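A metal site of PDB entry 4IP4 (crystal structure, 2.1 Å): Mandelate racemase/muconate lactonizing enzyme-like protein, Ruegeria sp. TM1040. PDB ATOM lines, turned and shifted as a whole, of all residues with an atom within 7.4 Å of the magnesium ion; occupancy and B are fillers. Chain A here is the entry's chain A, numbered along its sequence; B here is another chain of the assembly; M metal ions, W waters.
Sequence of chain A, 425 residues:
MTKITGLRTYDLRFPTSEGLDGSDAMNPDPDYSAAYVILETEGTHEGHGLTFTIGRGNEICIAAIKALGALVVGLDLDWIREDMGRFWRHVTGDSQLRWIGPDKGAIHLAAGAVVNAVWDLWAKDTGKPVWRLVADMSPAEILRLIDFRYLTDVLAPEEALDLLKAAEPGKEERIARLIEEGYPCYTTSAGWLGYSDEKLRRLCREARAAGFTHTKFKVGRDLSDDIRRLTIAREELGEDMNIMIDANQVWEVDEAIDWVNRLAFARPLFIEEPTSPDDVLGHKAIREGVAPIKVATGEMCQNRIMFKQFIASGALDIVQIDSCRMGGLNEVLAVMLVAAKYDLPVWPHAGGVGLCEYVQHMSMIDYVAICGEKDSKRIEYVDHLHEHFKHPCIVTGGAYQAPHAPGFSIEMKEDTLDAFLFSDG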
ATOM      1  N   ASP A  24      -0.144   7.005  -4.924  1.00  0.00           N
ATOM      2  CA  ASP A  24       1.071   6.271  -4.603  1.00  0.00           C
ATOM      3  C   ASP A  24       1.145   4.942  -5.346  1.00  0.00           C
ATOM      4  O   ASP A  24       0.297   4.619  -6.180  1.00  0.00           O
ATOM      5  CB  ASP A  24       1.209   6.082  -3.089  1.00  0.00           C
ATOM      6  CG  ASP A  24       0.092   5.228  -2.491  1.00  0.00           C
ATOM      7  OD1 ASP A  24      -0.120   4.095  -2.990  1.00  0.00           O
ATOM      8  OD2 ASP A  24      -0.564   5.683  -1.523  1.00  0.00           O
ATOM      9  N   TYR A 186       7.391  16.839   8.961  1.00  0.00           N
ATOM     10  CA  TYR A 186       7.874  16.686   7.605  1.00  0.00           C
ATOM     11  C   TYR A 186       6.726  16.718   6.621  1.00  0.00           C
ATOM     12  O   TYR A 186       5.587  16.443   6.976  1.00  0.00           O
ATOM     13  CB  TYR A 186       8.688  15.404   7.446  1.00  0.00           C
ATOM     14  CG  TYR A 186       7.899  14.101   7.414  1.00  0.00           C
ATOM     15  CD1 TYR A 186       7.392  13.592   6.226  1.00  0.00           C
ATOM     16  CD2 TYR A 186       7.690  13.350   8.584  1.00  0.00           C
ATOM     17  CE1 TYR A 186       6.689  12.396   6.191  1.00  0.00           C
ATOM     18  CE2 TYR A 186       6.991  12.139   8.557  1.00  0.00           C
ATOM     19  CZ  TYR A 186       6.490  11.674   7.358  1.00  0.00           C
ATOM     20  OH  TYR A 186       5.801  10.486   7.317  1.00  0.00           O
ATOM     21  N   THR A 188       4.958  15.526   2.887  1.00  0.00           N
ATOM     22  CA  THR A 188       4.852  14.525   1.831  1.00  0.00           C
ATOM     23  C   THR A 188       4.181  15.185   0.619  1.00  0.00           C
ATOM     24  O   THR A 188       3.971  14.556  -0.422  1.00  0.00           O
ATOM     25  CB  THR A 188       4.027  13.303   2.324  1.00  0.00           C
ATOM     26  OG1 THR A 188       4.558  12.840   3.576  1.00  0.00           O
ATOM     27  CG2 THR A 188       4.088  12.151   1.325  1.00  0.00           C
ATOM     28  N   TRP A 192       3.846  12.987  -4.121  1.00  0.00           N
ATOM     29  CA  TRP A 192       2.835  12.085  -4.683  1.00  0.00           C
ATOM     30  C   TRP A 192       3.242  11.564  -6.056  1.00  0.00           C
ATOM     31  O   TRP A 192       3.765  12.298  -6.902  1.00  0.00           O
ATOM     32  CB  TRP A 192       1.455  12.743  -4.765  1.00  0.00           C
ATOM     33  CG  TRP A 192       0.980  13.317  -3.452  1.00  0.00           C
ATOM     34  CD1 TRP A 192       0.718  14.634  -3.184  1.00  0.00           C
ATOM     35  CD2 TRP A 192       0.728  12.597  -2.235  1.00  0.00           C
ATOM     36  NE1 TRP A 192       0.313  14.767  -1.874  1.00  0.00           N
ATOM     37  CE2 TRP A 192       0.316  13.541  -1.273  1.00  0.00           C
ATOM     38  CE3 TRP A 192       0.817  11.254  -1.872  1.00  0.00           C
ATOM     39  CZ2 TRP A 192      -0.027  13.173   0.032  1.00  0.00           C
ATOM     40  CZ3 TRP A 192       0.479  10.898  -0.575  1.00  0.00           C
ATOM     41  CH2 TRP A 192       0.064  11.850   0.357  1.00  0.00           C
ATOM     42  N   LYS A 216       9.279  13.764   2.138  1.00  0.00           N
ATOM     43  CA  LYS A 216       9.059  12.371   1.772  1.00  0.00           C
ATOM     44  C   LYS A 216       8.500  12.212   0.358  1.00  0.00           C
ATOM     45  O   LYS A 216       7.708  13.035  -0.085  1.00  0.00           O
ATOM     46  CB  LYS A 216       8.134  11.680   2.787  1.00  0.00           C
ATOM     47  CG  LYS A 216       8.047  10.146   2.607  1.00  0.00           C
ATOM     48  CD  LYS A 216       7.342   9.494   3.807  1.00  0.00           C
ATOM     49  CE  LYS A 216       5.834   9.671   3.750  1.00  0.00           C
ATOM     50  NZ  LYS A 216       5.171   9.051   4.946  1.00  0.00           N
ATOM     51  N   LYS A 218       6.933   9.376  -2.692  1.00  0.00           N
ATOM     52  CA  LYS A 218       6.403   8.066  -3.027  1.00  0.00           C
ATOM     53  C   LYS A 218       7.286   7.392  -4.080  1.00  0.00           C
ATOM     54  O   LYS A 218       7.783   8.056  -5.006  1.00  0.00           O
ATOM     55  CB  LYS A 218       4.969   8.184  -3.555  1.00  0.00           C
ATOM     56  CG  LYS A 218       3.981   8.759  -2.555  1.00  0.00           C
ATOM     57  CD  LYS A 218       3.873   7.892  -1.317  1.00  0.00           C
ATOM     58  CE  LYS A 218       2.778   8.392  -0.375  1.00  0.00           C
ATOM     59  NZ  LYS A 218       2.487   7.448   0.753  1.00  0.00           N
ATOM     60  N   ILE A 245      11.542   7.896   1.639  1.00  0.00           N
ATOM     61  CA  ILE A 245      10.761   7.268   0.584  1.00  0.00           C
ATOM     62  C   ILE A 245       9.717   6.277   1.145  1.00  0.00           C
ATOM     63  O   ILE A 245       9.924   5.667   2.200  1.00  0.00           O
ATOM     64  CB  ILE A 245      11.661   6.579  -0.468  1.00  0.00           C
ATOM     65  CG1 ILE A 245      12.531   5.510   0.183  1.00  0.00           C
ATOM     66  CG2 ILE A 245      12.555   7.602  -1.186  1.00  0.00           C
ATOM     67  CD1 ILE A 245      13.511   4.839  -0.762  1.00  0.00           C
ATOM     68  N   ASP A 246       8.604   6.135   0.423  1.00  0.00           N
ATOM     69  CA  ASP A 246       7.450   5.344   0.876  1.00  0.00           C
ATOM     70  C   ASP A 246       6.960   4.478  -0.293  1.00  0.00           C
ATOM     71  O   ASP A 246       6.557   5.009  -1.336  1.00  0.00           O
ATOM     72  CB  ASP A 246       6.321   6.286   1.309  1.00  0.00           C
ATOM     73  CG  ASP A 246       5.156   5.565   1.980  1.00  0.00           C
ATOM     74  OD1 ASP A 246       5.070   4.314   1.908  1.00  0.00           O
ATOM     75  OD2 ASP A 246       4.305   6.269   2.586  1.00  0.00           O
ATOM     76  N   ALA A 247       6.973   3.162  -0.101  1.00  0.00           N
ATOM     77  CA  ALA A 247       6.619   2.216  -1.166  1.00  0.00           C
ATOM     78  C   ALA A 247       5.178   1.703  -1.050  1.00  0.00           C
ATOM     79  O   ALA A 247       4.704   0.952  -1.905  1.00  0.00           O
ATOM     80  CB  ALA A 247       7.583   1.039  -1.167  1.00  0.00           C
ATOM     81  N   ASN A 248       4.512   2.093   0.030  1.00  0.00           N
ATOM     82  CA  ASN A 248       3.129   1.700   0.253  1.00  0.00           C
ATOM     83  C   ASN A 248       2.822   0.202   0.119  1.00  0.00           C
ATOM     84  O   ASN A 248       1.804  -0.158  -0.450  1.00  0.00           O
ATOM     85  CB  ASN A 248       2.191   2.517  -0.654  1.00  0.00           C
ATOM     86  CG  ASN A 248       1.976   3.910  -0.122  1.00  0.00           C
ATOM     87  OD1 ASN A 248       2.754   4.832  -0.406  1.00  0.00           O
ATOM     88  ND2 ASN A 248       0.940   4.064   0.693  1.00  0.00           N
ATOM     89  N   GLU A 272       9.721   3.473   3.894  1.00  0.00           N
ATOM     90  CA  GLU A 272       8.474   3.258   4.618  1.00  0.00           C
ATOM     91  C   GLU A 272       7.610   2.198   3.930  1.00  0.00           C
ATOM     92  O   GLU A 272       7.493   2.180   2.700  1.00  0.00           O
ATOM     93  CB  GLU A 272       7.696   4.570   4.697  1.00  0.00           C
ATOM     94  CG  GLU A 272       6.278   4.441   5.237  1.00  0.00           C
ATOM     95  CD  GLU A 272       5.613   5.790   5.495  1.00  0.00           C
ATOM     96  OE1 GLU A 272       6.372   6.778   5.687  1.00  0.00           O
ATOM     97  OE2 GLU A 272       4.372   5.872   5.508  1.00  0.00           O
ATOM     98  N   GLU A 273       7.008   1.322   4.744  1.00  0.00           N
ATOM     99  CA  GLU A 273       6.174   0.227   4.224  1.00  0.00           C
ATOM    100  C   GLU A 273       6.748  -0.472   2.977  1.00  0.00           C
ATOM    101  O   GLU A 273       6.101  -0.511   1.927  1.00  0.00           O
ATOM    102  CB  GLU A 273       4.772   0.731   3.913  1.00  0.00           C
ATOM    103  CG  GLU A 273       4.010   1.177   5.135  1.00  0.00           C
ATOM    104  CD  GLU A 273       2.520   0.953   4.964  1.00  0.00           C
ATOM    105  OE1 GLU A 273       1.892   1.738   4.221  1.00  0.00           O
ATOM    106  OE2 GLU A 273       1.995  -0.037   5.538  1.00  0.00           O
ATOM    107  N   GLU A 299       1.336   2.748   9.465  1.00  0.00           N
ATOM    108  CA  GLU A 299       0.105   3.488   9.182  1.00  0.00           C
ATOM    109  C   GLU A 299      -1.101   2.561   9.037  1.00  0.00           C
ATOM    110  O   GLU A 299      -2.229   2.979   9.311  1.00  0.00           O
ATOM    111  CB  GLU A 299       0.249   4.375   7.956  1.00  0.00           C
ATOM    112  CG  GLU A 299       0.240   3.632   6.633  1.00  0.00           C
ATOM    113  CD  GLU A 299       0.592   4.553   5.484  1.00  0.00           C
ATOM    114  OE1 GLU A 299       1.631   5.248   5.581  1.00  0.00           O
ATOM    115  OE2 GLU A 299      -0.158   4.601   4.496  1.00  0.00           O
ATOM    116  N   GLN A 320       5.333   4.293  13.040  1.00  0.00           N
ATOM    117  CA  GLN A 320       4.400   5.242  12.427  1.00  0.00           C
ATOM    118  C   GLN A 320       2.940   4.956  12.774  1.00  0.00           C
ATOM    119  O   GLN A 320       2.203   4.428  11.976  1.00  0.00           O
ATOM    120  CB  GLN A 320       4.586   5.267  10.902  1.00  0.00           C
ATOM    121  CG  GLN A 320       5.993   5.679  10.479  1.00  0.00           C
ATOM    122  CD  GLN A 320       6.223   5.515   8.987  1.00  0.00           C
ATOM    123  OE1 GLN A 320       5.924   4.466   8.407  1.00  0.00           O
ATOM    124  NE2 GLN A 320       6.765   6.557   8.352  1.00  0.00           N
ATOM    125  N   HIS A 349       1.687   8.848  10.974  1.00  0.00           N
ATOM    126  CA  HIS A 349       1.109   8.994   9.637  1.00  0.00           C
ATOM    127  C   HIS A 349       0.094  10.133   9.630  1.00  0.00           C
ATOM    128  O   HIS A 349      -0.661  10.289  10.587  1.00  0.00           O
ATOM    129  CB  HIS A 349       0.411   7.688   9.241  1.00  0.00           C
ATOM    130  CG  HIS A 349      -0.313   7.750   7.928  1.00  0.00           C
ATOM    131  ND1 HIS A 349      -1.673   7.574   7.817  1.00  0.00           N
ATOM    132  CD2 HIS A 349       0.141   7.952   6.665  1.00  0.00           C
ATOM    133  CE1 HIS A 349      -2.032   7.680   6.549  1.00  0.00           C
ATOM    134  NE2 HIS A 349      -0.953   7.905   5.827  1.00  0.00           N
ATOM    135  N   ALA A 350       0.070  10.913   8.554  1.00  0.00           N
ATOM    136  CA  ALA A 350      -0.885  12.024   8.463  1.00  0.00           C
ATOM    137  C   ALA A 350      -1.437  12.203   7.044  1.00  0.00           C
ATOM    138  O   ALA A 350      -2.068  13.220   6.724  1.00  0.00           O
ATOM    139  CB  ALA A 350      -0.269  13.330   8.953  1.00  0.00           C
ATOM    140  N   GLY A 351      -1.206  11.193   6.204  1.00  0.00           N
ATOM    141  CA  GLY A 351      -1.624  11.236   4.816  1.00  0.00           C
ATOM    142  C   GLY A 351      -3.114  10.929   4.684  1.00  0.00           C
ATOM    143  O   GLY A 351      -3.488   9.798   4.364  1.00  0.00           O
ATOM    144  N   GLU A 380       4.262  13.494  10.325  1.00  0.00           N
ATOM    145  CA  GLU A 380       3.955  13.723   8.923  1.00  0.00           C
ATOM    146  C   GLU A 380       3.025  14.930   8.801  1.00  0.00           C
ATOM    147  O   GLU A 380       2.221  15.206   9.703  1.00  0.00           O
ATOM    148  CB  GLU A 380       3.325  12.487   8.283  1.00  0.00           C
ATOM    149  CG  GLU A 380       3.027  12.657   6.800  1.00  0.00           C
ATOM    150  CD  GLU A 380       2.774  11.344   6.074  1.00  0.00           C
ATOM    151  OE1 GLU A 380       2.274  10.384   6.721  1.00  0.00           O
ATOM    152  OE2 GLU A 380       3.083  11.275   4.866  1.00  0.00           O
ATOM    153  N   TRP B  99      -7.827  -0.734   1.599  1.00  0.00           N
ATOM    154  CA  TRP B  99      -7.596   0.190   2.715  1.00  0.00           C
ATOM    155  C   TRP B  99      -8.418  -0.229   3.947  1.00  0.00           C
ATOM    156  O   TRP B  99      -8.022   0.024   5.086  1.00  0.00           O
ATOM    157  CB  TRP B  99      -7.948   1.619   2.312  1.00  0.00           C
ATOM    158  CG  TRP B  99      -7.394   2.633   3.272  1.00  0.00           C
ATOM    159  CD1 TRP B  99      -7.954   3.049   4.444  1.00  0.00           C
ATOM    160  CD2 TRP B  99      -6.155   3.350   3.140  1.00  0.00           C
ATOM    161  NE1 TRP B  99      -7.145   3.981   5.056  1.00  0.00           N
ATOM    162  CE2 TRP B  99      -6.040   4.182   4.275  1.00  0.00           C
ATOM    163  CE3 TRP B  99      -5.151   3.376   2.169  1.00  0.00           C
ATOM    164  CZ2 TRP B  99      -4.943   5.021   4.462  1.00  0.00           C
ATOM    165  CZ3 TRP B  99      -4.061   4.203   2.373  1.00  0.00           C
ATOM    166  CH2 TRP B  99      -3.970   5.022   3.500  1.00  0.00           C
HETATM  167 MG    MG M   1       2.937   5.925   4.062  1.00  0.00          MG
HETATM  168  O   HOH W   1       2.578   8.007   4.652  1.00  0.00           O
HETATM  169  O   HOH W   2       1.196   6.094   2.956  1.00  0.00           O
HETATM  170  O   HOH W   3       2.993   3.989   3.402  1.00  0.00           O
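The side-chain carboxylate of Glu 272 is in salt-bridge range of the side-chain amino group of Lys 216.
The backbone carbonyl oxygen of Glu 272 sits at hydrogen-bond distance from the backbone NH of Ala 247 (3.0 Å).
The backbone NH (N) of Glu 272 lies within hydrogen-bond range of the backbone carbonyl oxygen (O) of Ile 245.
The side-chain carboxylate of Asp 246 lies close to the side-chain amino group of Lys 218 (2.8 Å).
The side-chain carboxylate (OD2) of Asp 246 sits close to the side-chain amino group (NZ) of Lys 216 (3.7 Å).
The side-chain carboxylate (OD1) of Asp 246 is in hydrogen-bond range of the backbone NH (N) of Asn 248.
NZ of Lys 218 lies within hydrogen-bond range of OD1 of Asn 248, 2.9 Å away.
The side-chain hydroxyl (OH) of Tyr 186 sits at hydrogen-bond distance from the side-chain amino group (NZ) of Lys 216.
Lys 216 touches the magnesium ion (NZ to MG, 3.9 Å).
Lys 218 touches the magnesium ion (NZ to MG, 3.7 Å).
Of the 19 residues printed, 5 come within 4 Å of the magnesium ion.
The magnesium ion is bound by OE2 of Glu 272, 2.0 Å away.
OD2 of Asp 246 is bound to the magnesium ion (2.0 Å).
Water W3 binds the magnesium ion (2.0 Å).
Water W2 binds the magnesium ion, at 2.1 Å.
The side-chain carboxylate (OE1) of Glu 299 binds the magnesium ion.
The magnesium ion is bound by water W1, at 2.2 Å.
The magnesium ion has six donor atoms within binding distance.
Water W1 lies within hydrogen-bond range of the side-chain amino group of Lys 216 (2.8 Å) and the side-chain carboxylate of Glu 380 (3.2 Å).
Water W2 lies within hydrogen-bond range of OE2 of Glu 299 (2.5 Å), NZ of Lys 218 (2.9 Å) and ND2 of Asn 248 (3.1 Å).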
